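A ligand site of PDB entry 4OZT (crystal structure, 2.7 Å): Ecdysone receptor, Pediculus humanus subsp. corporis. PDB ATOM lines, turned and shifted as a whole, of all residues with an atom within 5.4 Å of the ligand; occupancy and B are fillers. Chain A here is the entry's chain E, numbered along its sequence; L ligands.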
ATOM      1  N   GLU A  23     -15.255 -14.540  41.240  1.00  0.00           N
ATOM      2  CA  GLU A  23     -15.562 -13.716  40.079  1.00  0.00           C
ATOM      3  C   GLU A  23     -14.450 -13.726  39.048  1.00  0.00           C
ATOM      4  O   GLU A  23     -14.709 -13.647  37.846  1.00  0.00           O
ATOM      5  CB  GLU A  23     -15.826 -12.283  40.535  1.00  0.00           C
ATOM      6  CG  GLU A  23     -16.336 -11.370  39.436  1.00  0.00           C
ATOM      7  CD  GLU A  23     -17.367 -10.399  39.960  1.00  0.00           C
ATOM      8  OE1 GLU A  23     -17.164  -9.856  41.073  1.00  0.00           O
ATOM      9  OE2 GLU A  23     -18.384 -10.196  39.267  1.00  0.00           O
ATOM     10  N   GLN A  24     -13.214 -13.800  39.514  1.00  0.00           N
ATOM     11  CA  GLN A  24     -12.060 -13.718  38.617  1.00  0.00           C
ATOM     12  C   GLN A  24     -11.128 -14.915  38.722  1.00  0.00           C
ATOM     13  O   GLN A  24     -10.910 -15.455  39.801  1.00  0.00           O
ATOM     14  CB  GLN A  24     -11.277 -12.421  38.880  1.00  0.00           C
ATOM     15  CG  GLN A  24     -12.010 -11.152  38.505  1.00  0.00           C
ATOM     16  CD  GLN A  24     -11.098 -10.102  37.895  1.00  0.00           C
ATOM     17  OE1 GLN A  24      -9.883 -10.306  37.791  1.00  0.00           O
ATOM     18  NE2 GLN A  24     -11.678  -8.983  37.475  1.00  0.00           N
ATOM     19  N   PRO A  25     -10.561 -15.326  37.577  1.00  0.00           N
ATOM     20  CA  PRO A  25      -9.534 -16.373  37.549  1.00  0.00           C
ATOM     21  C   PRO A  25      -8.293 -15.880  38.257  1.00  0.00           C
ATOM     22  O   PRO A  25      -8.084 -14.668  38.312  1.00  0.00           O
ATOM     23  CB  PRO A  25      -9.223 -16.531  36.058  1.00  0.00           C
ATOM     24  CG  PRO A  25     -10.412 -15.961  35.334  1.00  0.00           C
ATOM     25  CD  PRO A  25     -10.914 -14.856  36.214  1.00  0.00           C
ATOM     26  N   ILE A  51     -10.422 -16.164  24.202  1.00  0.00           N
ATOM     27  CA  ILE A  51     -11.850 -16.365  24.482  1.00  0.00           C
ATOM     28  C   ILE A  51     -12.167 -17.759  25.025  1.00  0.00           C
ATOM     29  O   ILE A  51     -12.781 -17.898  26.102  1.00  0.00           O
ATOM     30  CB  ILE A  51     -12.708 -16.047  23.247  1.00  0.00           C
ATOM     31  CG1 ILE A  51     -12.697 -14.546  22.971  1.00  0.00           C
ATOM     32  CG2 ILE A  51     -14.132 -16.524  23.434  1.00  0.00           C
ATOM     33  CD1 ILE A  51     -13.366 -14.161  21.667  1.00  0.00           C
ATOM     34  N   THR A  52     -11.719 -18.795  24.311  1.00  0.00           N
ATOM     35  CA  THR A  52     -11.996 -20.171  24.727  1.00  0.00           C
ATOM     36  C   THR A  52     -11.267 -20.594  26.020  1.00  0.00           C
ATOM     37  O   THR A  52     -11.879 -21.129  26.973  1.00  0.00           O
ATOM     38  CB  THR A  52     -11.701 -21.159  23.587  1.00  0.00           C
ATOM     39  OG1 THR A  52     -10.390 -20.909  23.070  1.00  0.00           O
ATOM     40  CG2 THR A  52     -12.700 -20.978  22.462  1.00  0.00           C
ATOM     41  N   ILE A  54      -9.970 -18.762  28.383  1.00  0.00           N
ATOM     42  CA  ILE A  54     -10.488 -18.072  29.563  1.00  0.00           C
ATOM     43  C   ILE A  54     -11.876 -18.596  29.906  1.00  0.00           C
ATOM     44  O   ILE A  54     -12.201 -18.759  31.093  1.00  0.00           O
ATOM     45  CB  ILE A  54     -10.527 -16.531  29.399  1.00  0.00           C
ATOM     46  CG1 ILE A  54      -9.105 -15.978  29.268  1.00  0.00           C
ATOM     47  CG2 ILE A  54     -11.191 -15.886  30.593  1.00  0.00           C
ATOM     48  CD1 ILE A  54      -9.076 -14.470  29.113  1.00  0.00           C
ATOM     49  N   THR A  55     -12.682 -18.891  28.879  1.00  0.00           N
ATOM     50  CA  THR A  55     -14.008 -19.460  29.122  1.00  0.00           C
ATOM     51  C   THR A  55     -13.932 -20.745  29.961  1.00  0.00           C
ATOM     52  O   THR A  55     -14.808 -20.999  30.800  1.00  0.00           O
ATOM     53  CB  THR A  55     -14.778 -19.696  27.810  1.00  0.00           C
ATOM     54  OG1 THR A  55     -14.881 -18.469  27.091  1.00  0.00           O
ATOM     55  CG2 THR A  55     -16.170 -20.238  28.094  1.00  0.00           C
ATOM     56  N   THR A  58     -13.666 -19.616  33.447  1.00  0.00           N
ATOM     57  CA  THR A  58     -14.988 -19.105  33.791  1.00  0.00           C
ATOM     58  C   THR A  58     -15.912 -20.239  34.238  1.00  0.00           C
ATOM     59  O   THR A  58     -16.577 -20.134  35.272  1.00  0.00           O
ATOM     60  CB  THR A  58     -15.628 -18.388  32.597  1.00  0.00           C
ATOM     61  OG1 THR A  58     -14.798 -17.300  32.187  1.00  0.00           O
ATOM     62  CG2 THR A  58     -17.010 -17.877  32.972  1.00  0.00           C
ATOM     63  N   LEU A  61     -14.924 -21.447  37.647  1.00  0.00           N
ATOM     64  CA  LEU A  61     -15.396 -20.484  38.635  1.00  0.00           C
ATOM     65  C   LEU A  61     -16.883 -20.687  38.917  1.00  0.00           C
ATOM     66  O   LEU A  61     -17.311 -20.651  40.079  1.00  0.00           O
ATOM     67  CB  LEU A  61     -15.141 -19.053  38.170  1.00  0.00           C
ATOM     68  CG  LEU A  61     -13.696 -18.586  37.991  1.00  0.00           C
ATOM     69  CD1 LEU A  61     -13.670 -17.154  37.501  1.00  0.00           C
ATOM     70  CD2 LEU A  61     -12.920 -18.716  39.291  1.00  0.00           C
ATOM     71  N   MET A  92     -22.786 -18.153  32.737  1.00  0.00           N
ATOM     72  CA  MET A  92     -21.746 -17.495  31.947  1.00  0.00           C
ATOM     73  C   MET A  92     -22.275 -16.211  31.305  1.00  0.00           C
ATOM     74  O   MET A  92     -21.574 -15.199  31.285  1.00  0.00           O
ATOM     75  CB  MET A  92     -21.211 -18.478  30.897  1.00  0.00           C
ATOM     76  CG  MET A  92     -20.161 -17.928  29.980  1.00  0.00           C
ATOM     77  SD  MET A  92     -19.596 -19.200  28.828  1.00  0.00           S
ATOM     78  CE  MET A  92     -21.078 -19.489  27.869  1.00  0.00           C
ATOM     79  N   MET A  93     -23.506 -16.253  30.786  1.00  0.00           N
ATOM     80  CA  MET A  93     -24.115 -15.032  30.249  1.00  0.00           C
ATOM     81  C   MET A  93     -24.279 -13.941  31.301  1.00  0.00           C
ATOM     82  O   MET A  93     -24.057 -12.750  31.019  1.00  0.00           O
ATOM     83  CB  MET A  93     -25.466 -15.341  29.598  1.00  0.00           C
ATOM     84  CG  MET A  93     -25.379 -16.308  28.428  1.00  0.00           C
ATOM     85  SD  MET A  93     -24.338 -15.661  27.130  1.00  0.00           S
ATOM     86  CE  MET A  93     -24.180 -17.105  26.079  1.00  0.00           C
ATOM     87  N   ARG A  95     -22.398 -13.583  34.124  1.00  0.00           N
ATOM     88  CA  ARG A  95     -21.046 -13.125  34.418  1.00  0.00           C
ATOM     89  C   ARG A  95     -20.561 -12.156  33.352  1.00  0.00           C
ATOM     90  O   ARG A  95     -19.964 -11.127  33.648  1.00  0.00           O
ATOM     91  CB  ARG A  95     -20.100 -14.320  34.527  1.00  0.00           C
ATOM     92  CG  ARG A  95     -20.271 -15.131  35.782  1.00  0.00           C
ATOM     93  CD  ARG A  95     -19.449 -16.402  35.728  1.00  0.00           C
ATOM     94  NE  ARG A  95     -19.257 -16.977  37.047  1.00  0.00           N
ATOM     95  CZ  ARG A  95     -18.230 -16.673  37.830  1.00  0.00           C
ATOM     96  NH1 ARG A  95     -17.317 -15.808  37.420  1.00  0.00           N
ATOM     97  NH2 ARG A  95     -18.121 -17.240  39.018  1.00  0.00           N
ATOM     98  N   MET A  96     -20.833 -12.500  32.096  1.00  0.00           N
ATOM     99  CA  MET A  96     -20.489 -11.623  30.989  1.00  0.00           C
ATOM    100  C   MET A  96     -21.187 -10.273  31.124  1.00  0.00           C
ATOM    101  O   MET A  96     -20.544  -9.224  31.005  1.00  0.00           O
ATOM    102  CB  MET A  96     -20.856 -12.265  29.657  1.00  0.00           C
ATOM    103  CG  MET A  96     -20.952 -11.274  28.524  1.00  0.00           C
ATOM    104  SD  MET A  96     -21.987 -11.903  27.199  1.00  0.00           S
ATOM    105  CE  MET A  96     -20.768 -12.023  25.904  1.00  0.00           C
ATOM    106  N   ARG A  99     -19.709  -7.542  33.257  1.00  0.00           N
ATOM    107  CA  ARG A  99     -18.459  -6.900  32.834  1.00  0.00           C
ATOM    108  C   ARG A  99     -18.640  -6.049  31.582  1.00  0.00           C
ATOM    109  O   ARG A  99     -17.670  -5.705  30.900  1.00  0.00           O
ATOM    110  CB  ARG A  99     -17.374  -7.958  32.598  1.00  0.00           C
ATOM    111  CG  ARG A  99     -17.029  -8.772  33.830  1.00  0.00           C
ATOM    112  CD  ARG A  99     -16.139  -7.988  34.764  1.00  0.00           C
ATOM    113  NE  ARG A  99     -14.753  -8.001  34.290  1.00  0.00           N
ATOM    114  CZ  ARG A  99     -13.786  -7.236  34.790  1.00  0.00           C
ATOM    115  NH1 ARG A  99     -14.048  -6.371  35.750  1.00  0.00           N
ATOM    116  NH2 ARG A  99     -12.558  -7.322  34.302  1.00  0.00           N
ATOM    117  N   ILE A 107     -17.128  -5.860  26.217  1.00  0.00           N
ATOM    118  CA  ILE A 107     -16.964  -6.650  27.426  1.00  0.00           C
ATOM    119  C   ILE A 107     -15.511  -6.563  27.873  1.00  0.00           C
ATOM    120  O   ILE A 107     -14.597  -6.783  27.080  1.00  0.00           O
ATOM    121  CB  ILE A 107     -17.351  -8.109  27.205  1.00  0.00           C
ATOM    122  CG1 ILE A 107     -18.854  -8.219  26.976  1.00  0.00           C
ATOM    123  CG2 ILE A 107     -16.962  -8.948  28.394  1.00  0.00           C
ATOM    124  CD1 ILE A 107     -19.211  -8.926  25.711  1.00  0.00           C
ATOM    125  N   LEU A 108     -15.308  -6.230  29.148  1.00  0.00           N
ATOM    126  CA  LEU A 108     -13.973  -6.101  29.710  1.00  0.00           C
ATOM    127  C   LEU A 108     -13.552  -7.412  30.351  1.00  0.00           C
ATOM    128  O   LEU A 108     -14.130  -7.809  31.371  1.00  0.00           O
ATOM    129  CB  LEU A 108     -13.927  -4.973  30.737  1.00  0.00           C
ATOM    130  CG  LEU A 108     -12.577  -4.633  31.375  1.00  0.00           C
ATOM    131  CD1 LEU A 108     -11.621  -4.093  30.321  1.00  0.00           C
ATOM    132  CD2 LEU A 108     -12.746  -3.651  32.516  1.00  0.00           C
ATOM    133  N   PHE A 109     -12.567  -8.095  29.771  1.00  0.00           N
ATOM    134  CA  PHE A 109     -12.143  -9.399  30.294  1.00  0.00           C
ATOM    135  C   PHE A 109     -11.331  -9.265  31.573  1.00  0.00           C
ATOM    136  O   PHE A 109     -10.931  -8.165  31.943  1.00  0.00           O
ATOM    137  CB  PHE A 109     -11.352 -10.184  29.254  1.00  0.00           C
ATOM    138  CG  PHE A 109     -12.181 -10.780  28.162  1.00  0.00           C
ATOM    139  CD1 PHE A 109     -13.514 -10.410  27.985  1.00  0.00           C
ATOM    140  CD2 PHE A 109     -11.636 -11.722  27.303  1.00  0.00           C
ATOM    141  CE1 PHE A 109     -14.279 -10.969  26.966  1.00  0.00           C
ATOM    142  CE2 PHE A 109     -12.391 -12.280  26.274  1.00  0.00           C
ATOM    143  CZ  PHE A 109     -13.714 -11.898  26.110  1.00  0.00           C
ATOM    144  N   ALA A 110     -11.085 -10.385  32.238  1.00  0.00           N
ATOM    145  CA  ALA A 110     -10.395 -10.386  33.533  1.00  0.00           C
ATOM    146  C   ALA A 110      -8.955  -9.887  33.438  1.00  0.00           C
ATOM    147  O   ALA A 110      -8.351  -9.524  34.452  1.00  0.00           O
ATOM    148  CB  ALA A 110     -10.449 -11.771  34.159  1.00  0.00           C
ATOM    149  N   ASN A 111      -8.424  -9.851  32.224  1.00  0.00           N
ATOM    150  CA  ASN A 111      -7.078  -9.331  31.980  1.00  0.00           C
ATOM    151  C   ASN A 111      -7.078  -7.856  31.595  1.00  0.00           C
ATOM    152  O   ASN A 111      -6.072  -7.344  31.091  1.00  0.00           O
ATOM    153  CB  ASN A 111      -6.379 -10.153  30.888  1.00  0.00           C
ATOM    154  CG  ASN A 111      -7.186 -10.220  29.591  1.00  0.00           C
ATOM    155  OD1 ASN A 111      -8.142  -9.469  29.396  1.00  0.00           O
ATOM    156  ND2 ASN A 111      -6.797 -11.128  28.696  1.00  0.00           N
ATOM    157  N   TYR A 120     -14.727 -10.316  18.663  1.00  0.00           N
ATOM    158  CA  TYR A 120     -15.462 -11.562  18.471  1.00  0.00           C
ATOM    159  C   TYR A 120     -15.583 -11.964  17.007  1.00  0.00           C
ATOM    160  O   TYR A 120     -15.415 -13.136  16.669  1.00  0.00           O
ATOM    161  CB  TYR A 120     -16.844 -11.460  19.112  1.00  0.00           C
ATOM    162  CG  TYR A 120     -16.845 -11.652  20.605  1.00  0.00           C
ATOM    163  CD1 TYR A 120     -16.562 -10.597  21.466  1.00  0.00           C
ATOM    164  CD2 TYR A 120     -17.138 -12.893  21.159  1.00  0.00           C
ATOM    165  CE1 TYR A 120     -16.554 -10.770  22.841  1.00  0.00           C
ATOM    166  CE2 TYR A 120     -17.136 -13.078  22.534  1.00  0.00           C
ATOM    167  CZ  TYR A 120     -16.847 -12.019  23.372  1.00  0.00           C
ATOM    168  OH  TYR A 120     -16.854 -12.210  24.727  1.00  0.00           O
ATOM    169  N   MET A 125     -16.432 -15.560  15.790  1.00  0.00           N
ATOM    170  CA  MET A 125     -17.659 -15.638  16.554  1.00  0.00           C
ATOM    171  C   MET A 125     -18.512 -14.385  16.350  1.00  0.00           C
ATOM    172  O   MET A 125     -18.942 -13.760  17.317  1.00  0.00           O
ATOM    173  CB  MET A 125     -17.351 -15.817  18.044  1.00  0.00           C
ATOM    174  CG  MET A 125     -16.435 -16.991  18.361  1.00  0.00           C
ATOM    175  SD  MET A 125     -16.060 -17.113  20.123  1.00  0.00           S
ATOM    176  CE  MET A 125     -15.574 -18.830  20.256  1.00  0.00           C
ATOM    177  N   THR A 128     -23.121 -14.235  16.692  1.00  0.00           N
ATOM    178  CA  THR A 128     -23.837 -14.349  17.967  1.00  0.00           C
ATOM    179  C   THR A 128     -23.572 -13.138  18.888  1.00  0.00           C
ATOM    180  O   THR A 128     -24.376 -12.799  19.799  1.00  0.00           O
ATOM    181  CB  THR A 128     -23.412 -15.691  18.634  1.00  0.00           C
ATOM    182  OG1 THR A 128     -24.445 -16.665  18.424  1.00  0.00           O
ATOM    183  CG2 THR A 128     -23.142 -15.552  20.113  1.00  0.00           C
ATOM    184  N   LEU A 132     -25.380 -11.282  22.181  1.00  0.00           N
ATOM    185  CA  LEU A 132     -24.694 -11.202  23.483  1.00  0.00           C
ATOM    186  C   LEU A 132     -24.662  -9.774  24.041  1.00  0.00           C
ATOM    187  O   LEU A 132     -25.082  -9.513  25.194  1.00  0.00           O
ATOM    188  CB  LEU A 132     -23.264 -11.743  23.350  1.00  0.00           C
ATOM    189  CG  LEU A 132     -23.131 -13.204  22.928  1.00  0.00           C
ATOM    190  CD1 LEU A 132     -21.669 -13.649  22.932  1.00  0.00           C
ATOM    191  CD2 LEU A 132     -23.965 -14.107  23.814  1.00  0.00           C
ATOM    192  N   ASN A 214     -25.566 -20.479  22.445  1.00  0.00           N
ATOM    193  CA  ASN A 214     -24.203 -20.829  22.798  1.00  0.00           C
ATOM    194  C   ASN A 214     -23.934 -22.287  22.472  1.00  0.00           C
ATOM    195  O   ASN A 214     -22.800 -22.691  22.209  1.00  0.00           O
ATOM    196  CB  ASN A 214     -23.931 -20.548  24.271  1.00  0.00           C
ATOM    197  CG  ASN A 214     -22.486 -20.818  24.644  1.00  0.00           C
ATOM    198  OD1 ASN A 214     -22.167 -21.889  25.160  1.00  0.00           O
ATOM    199  ND2 ASN A 214     -21.623 -19.864  24.378  1.00  0.00           N
ATOM    200  N   MET A 217     -23.313 -22.391  18.527  1.00  0.00           N
ATOM    201  CA  MET A 217     -21.961 -22.231  18.030  1.00  0.00           C
ATOM    202  C   MET A 217     -21.423 -23.670  17.866  1.00  0.00           C
ATOM    203  O   MET A 217     -22.197 -24.592  17.611  1.00  0.00           O
ATOM    204  CB  MET A 217     -21.134 -21.368  18.971  1.00  0.00           C
ATOM    205  CG  MET A 217     -19.866 -20.786  18.371  1.00  0.00           C
ATOM    206  SD  MET A 217     -19.700 -19.022  18.688  1.00  0.00           S
ATOM    207  CE  MET A 217     -20.823 -18.320  17.463  1.00  0.00           C
ATOM    208  N   LEU A 228     -13.640 -26.104  19.682  1.00  0.00           N
ATOM    209  CA  LEU A 228     -13.802 -25.842  21.103  1.00  0.00           C
ATOM    210  C   LEU A 228     -12.847 -26.720  21.885  1.00  0.00           C
ATOM    211  O   LEU A 228     -12.635 -27.876  21.514  1.00  0.00           O
ATOM    212  CB  LEU A 228     -15.225 -26.183  21.557  1.00  0.00           C
ATOM    213  CG  LEU A 228     -16.333 -25.155  21.429  1.00  0.00           C
ATOM    214  CD1 LEU A 228     -17.564 -25.684  22.141  1.00  0.00           C
ATOM    215  CD2 LEU A 228     -15.893 -23.839  22.023  1.00  0.00           C
ATOM    216  N   LEU A 232     -15.083 -27.903  27.241  1.00  0.00           N
ATOM    217  CA  LEU A 232     -16.295 -27.163  26.880  1.00  0.00           C
ATOM    218  C   LEU A 232     -17.203 -27.977  25.971  1.00  0.00           C
ATOM    219  O   LEU A 232     -18.429 -27.947  26.102  1.00  0.00           O
ATOM    220  CB  LEU A 232     -15.930 -25.831  26.217  1.00  0.00           C
ATOM    221  CG  LEU A 232     -15.122 -24.869  27.083  1.00  0.00           C
ATOM    222  CD1 LEU A 232     -14.844 -23.570  26.346  1.00  0.00           C
ATOM    223  CD2 LEU A 232     -15.869 -24.603  28.377  1.00  0.00           C
ATOM    224  N   TRP A 236     -20.996 -29.015  27.317  1.00  0.00           N
ATOM    225  CA  TRP A 236     -22.170 -28.508  26.593  1.00  0.00           C
ATOM    226  C   TRP A 236     -22.745 -29.469  25.575  1.00  0.00           C
ATOM    227  O   TRP A 236     -23.476 -29.058  24.671  1.00  0.00           O
ATOM    228  CB  TRP A 236     -21.846 -27.171  25.941  1.00  0.00           C
ATOM    229  CG  TRP A 236     -21.628 -26.102  26.983  1.00  0.00           C
ATOM    230  CD1 TRP A 236     -22.205 -26.035  28.217  1.00  0.00           C
ATOM    231  CD2 TRP A 236     -20.757 -24.959  26.881  1.00  0.00           C
ATOM    232  NE1 TRP A 236     -21.742 -24.923  28.886  1.00  0.00           N
ATOM    233  CE2 TRP A 236     -20.857 -24.244  28.088  1.00  0.00           C
ATOM    234  CE3 TRP A 236     -19.892 -24.473  25.885  1.00  0.00           C
ATOM    235  CZ2 TRP A 236     -20.127 -23.057  28.322  1.00  0.00           C
ATOM    236  CZ3 TRP A 236     -19.177 -23.294  26.122  1.00  0.00           C
ATOM    237  CH2 TRP A 236     -19.290 -22.604  27.331  1.00  0.00           C
HETATM  238  C1  LIG L   1     -14.274 -12.889  32.314  1.00  0.00           C
HETATM  239  C2  LIG L   1     -15.754 -12.908  31.967  1.00  0.00           C
HETATM  240  C3  LIG L   1     -16.468 -12.822  33.292  1.00  0.00           C
HETATM  241  C4  LIG L   1     -16.179 -14.003  34.198  1.00  0.00           C
HETATM  242  C5  LIG L   1     -14.680 -14.189  34.452  1.00  0.00           C
HETATM  243  C6  LIG L   1     -13.824 -14.014  33.231  1.00  0.00           C
HETATM  244  C7  LIG L   1     -16.190 -14.094  31.095  1.00  0.00           C
HETATM  245  C8  LIG L   1     -15.988 -11.598  31.290  1.00  0.00           C
HETATM  246  C9  LIG L   1     -17.667 -14.093  30.727  1.00  0.00           C
HETATM  247  C10 LIG L   1     -15.315 -14.212  29.893  1.00  0.00           C
HETATM  248  C11 LIG L   1     -18.065 -14.978  29.549  1.00  0.00           C
HETATM  249  C12 LIG L   1     -15.814 -14.955  28.679  1.00  0.00           C
HETATM  250  C13 LIG L   1     -17.249 -14.683  28.296  1.00  0.00           C
HETATM  251  C14 LIG L   1     -17.342 -13.216  27.929  1.00  0.00           C
HETATM  252  C15 LIG L   1     -17.391 -15.618  27.088  1.00  0.00           C
HETATM  253  O1  LIG L   1     -15.648 -16.327  29.011  1.00  0.00           O
HETATM  254  C16 LIG L   1     -15.092 -14.807  27.368  1.00  0.00           C
HETATM  255  C17 LIG L   1     -18.604 -15.527  26.103  1.00  0.00           C
HETATM  256  C18 LIG L   1     -16.047 -15.491  26.392  1.00  0.00           C
HETATM  257  C19 LIG L   1     -18.495 -16.506  24.913  1.00  0.00           C
HETATM  258  O2  LIG L   1     -18.581 -14.288  25.432  1.00  0.00           O
HETATM  259  C20 LIG L   1     -19.956 -15.660  26.779  1.00  0.00           C
HETATM  260  C21 LIG L   1     -13.469 -13.117  31.065  1.00  0.00           C
HETATM  261  C22 LIG L   1     -14.053 -13.769  29.880  1.00  0.00           C
HETATM  262  O3  LIG L   1     -14.155 -13.286  35.406  1.00  0.00           O
HETATM  263  O4  LIG L   1     -16.912 -13.827  35.424  1.00  0.00           O
HETATM  264  O5  LIG L   1     -19.446 -16.240  23.876  1.00  0.00           O
HETATM  265  C23 LIG L   1     -18.595 -17.981  25.156  1.00  0.00           C
HETATM  266  C24 LIG L   1     -18.012 -18.552  23.878  1.00  0.00           C
HETATM  267  C25 LIG L   1     -17.525 -19.944  24.150  1.00  0.00           C
HETATM  268  C26 LIG L   1     -16.017 -20.073  24.377  1.00  0.00           C
HETATM  269  C27 LIG L   1     -18.138 -20.863  23.124  1.00  0.00           C
HETATM  270  O6  LIG L   1     -12.267 -12.882  31.054  1.00  0.00           O
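Residues that only touch the ligand: Gln 24 (3.9 Å), Pro 25 (3.7 Å), Ile 51 (3.7 Å), Thr 52 (3.9 Å), Ile 54 (3.2 Å), Met 92 (3.6 Å), Met 96 (3.2 Å), Arg 99 (3.9 Å), Phe 109 (3.4 Å), Leu 132 (3.5 Å), Asn 214 (3.6 Å), Leu 228 (3.9 Å) and Trp 236 (3.997 Å).
Within 4 Å of the ligand: Glu 23, Gln 24, Pro 25, Ile 51, Thr 52, Ile 54, Thr 55, Thr 58, Met 92, Arg 95, Met 96, Arg 99, Phe 109, Ala 110, Tyr 120, Leu 132, Asn 214, Leu 228 and Trp 236.
O of Glu 23 sits at hydrogen-bond distance from NH1 of Arg 95 (3.4 Å).
The backbone NH (N) of Met 125 lies within hydrogen-bond range of the backbone carbonyl oxygen (O) of Tyr 120 (2.8 Å).
O of Ile 54 is in hydrogen-bond range of OG1 of Thr 58 (3.2 Å).
The guanidinium group of Arg 99 lies within hydrogen-bond range of the backbone carbonyl oxygen of Phe 109 (3.0 Å).
N of Leu 108 lies within hydrogen-bond range of O of Arg 99.
An oxygen (O3) of the ligand sits at hydrogen-bond distance from the backbone carbonyl oxygen (O) of Glu 23, at 2.5 Å.
O2 of the ligand lies within hydrogen-bond range of OH of Tyr 120.
O4 of the ligand lies within hydrogen-bond range of NH1 of Arg 95 (2.8 Å).
The side-chain hydroxyl (OG1) of Thr 55 lies within hydrogen-bond range of an oxygen (O1) of the ligand, 3.0 Å away.
N of Ala 110 is in hydrogen-bond range of O6 of the ligand (3.0 Å).
The side-chain hydroxyl (OG1) of Thr 58 sits at hydrogen-bond distance from an oxygen (O1) of the ligand, at 3.4 Å.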
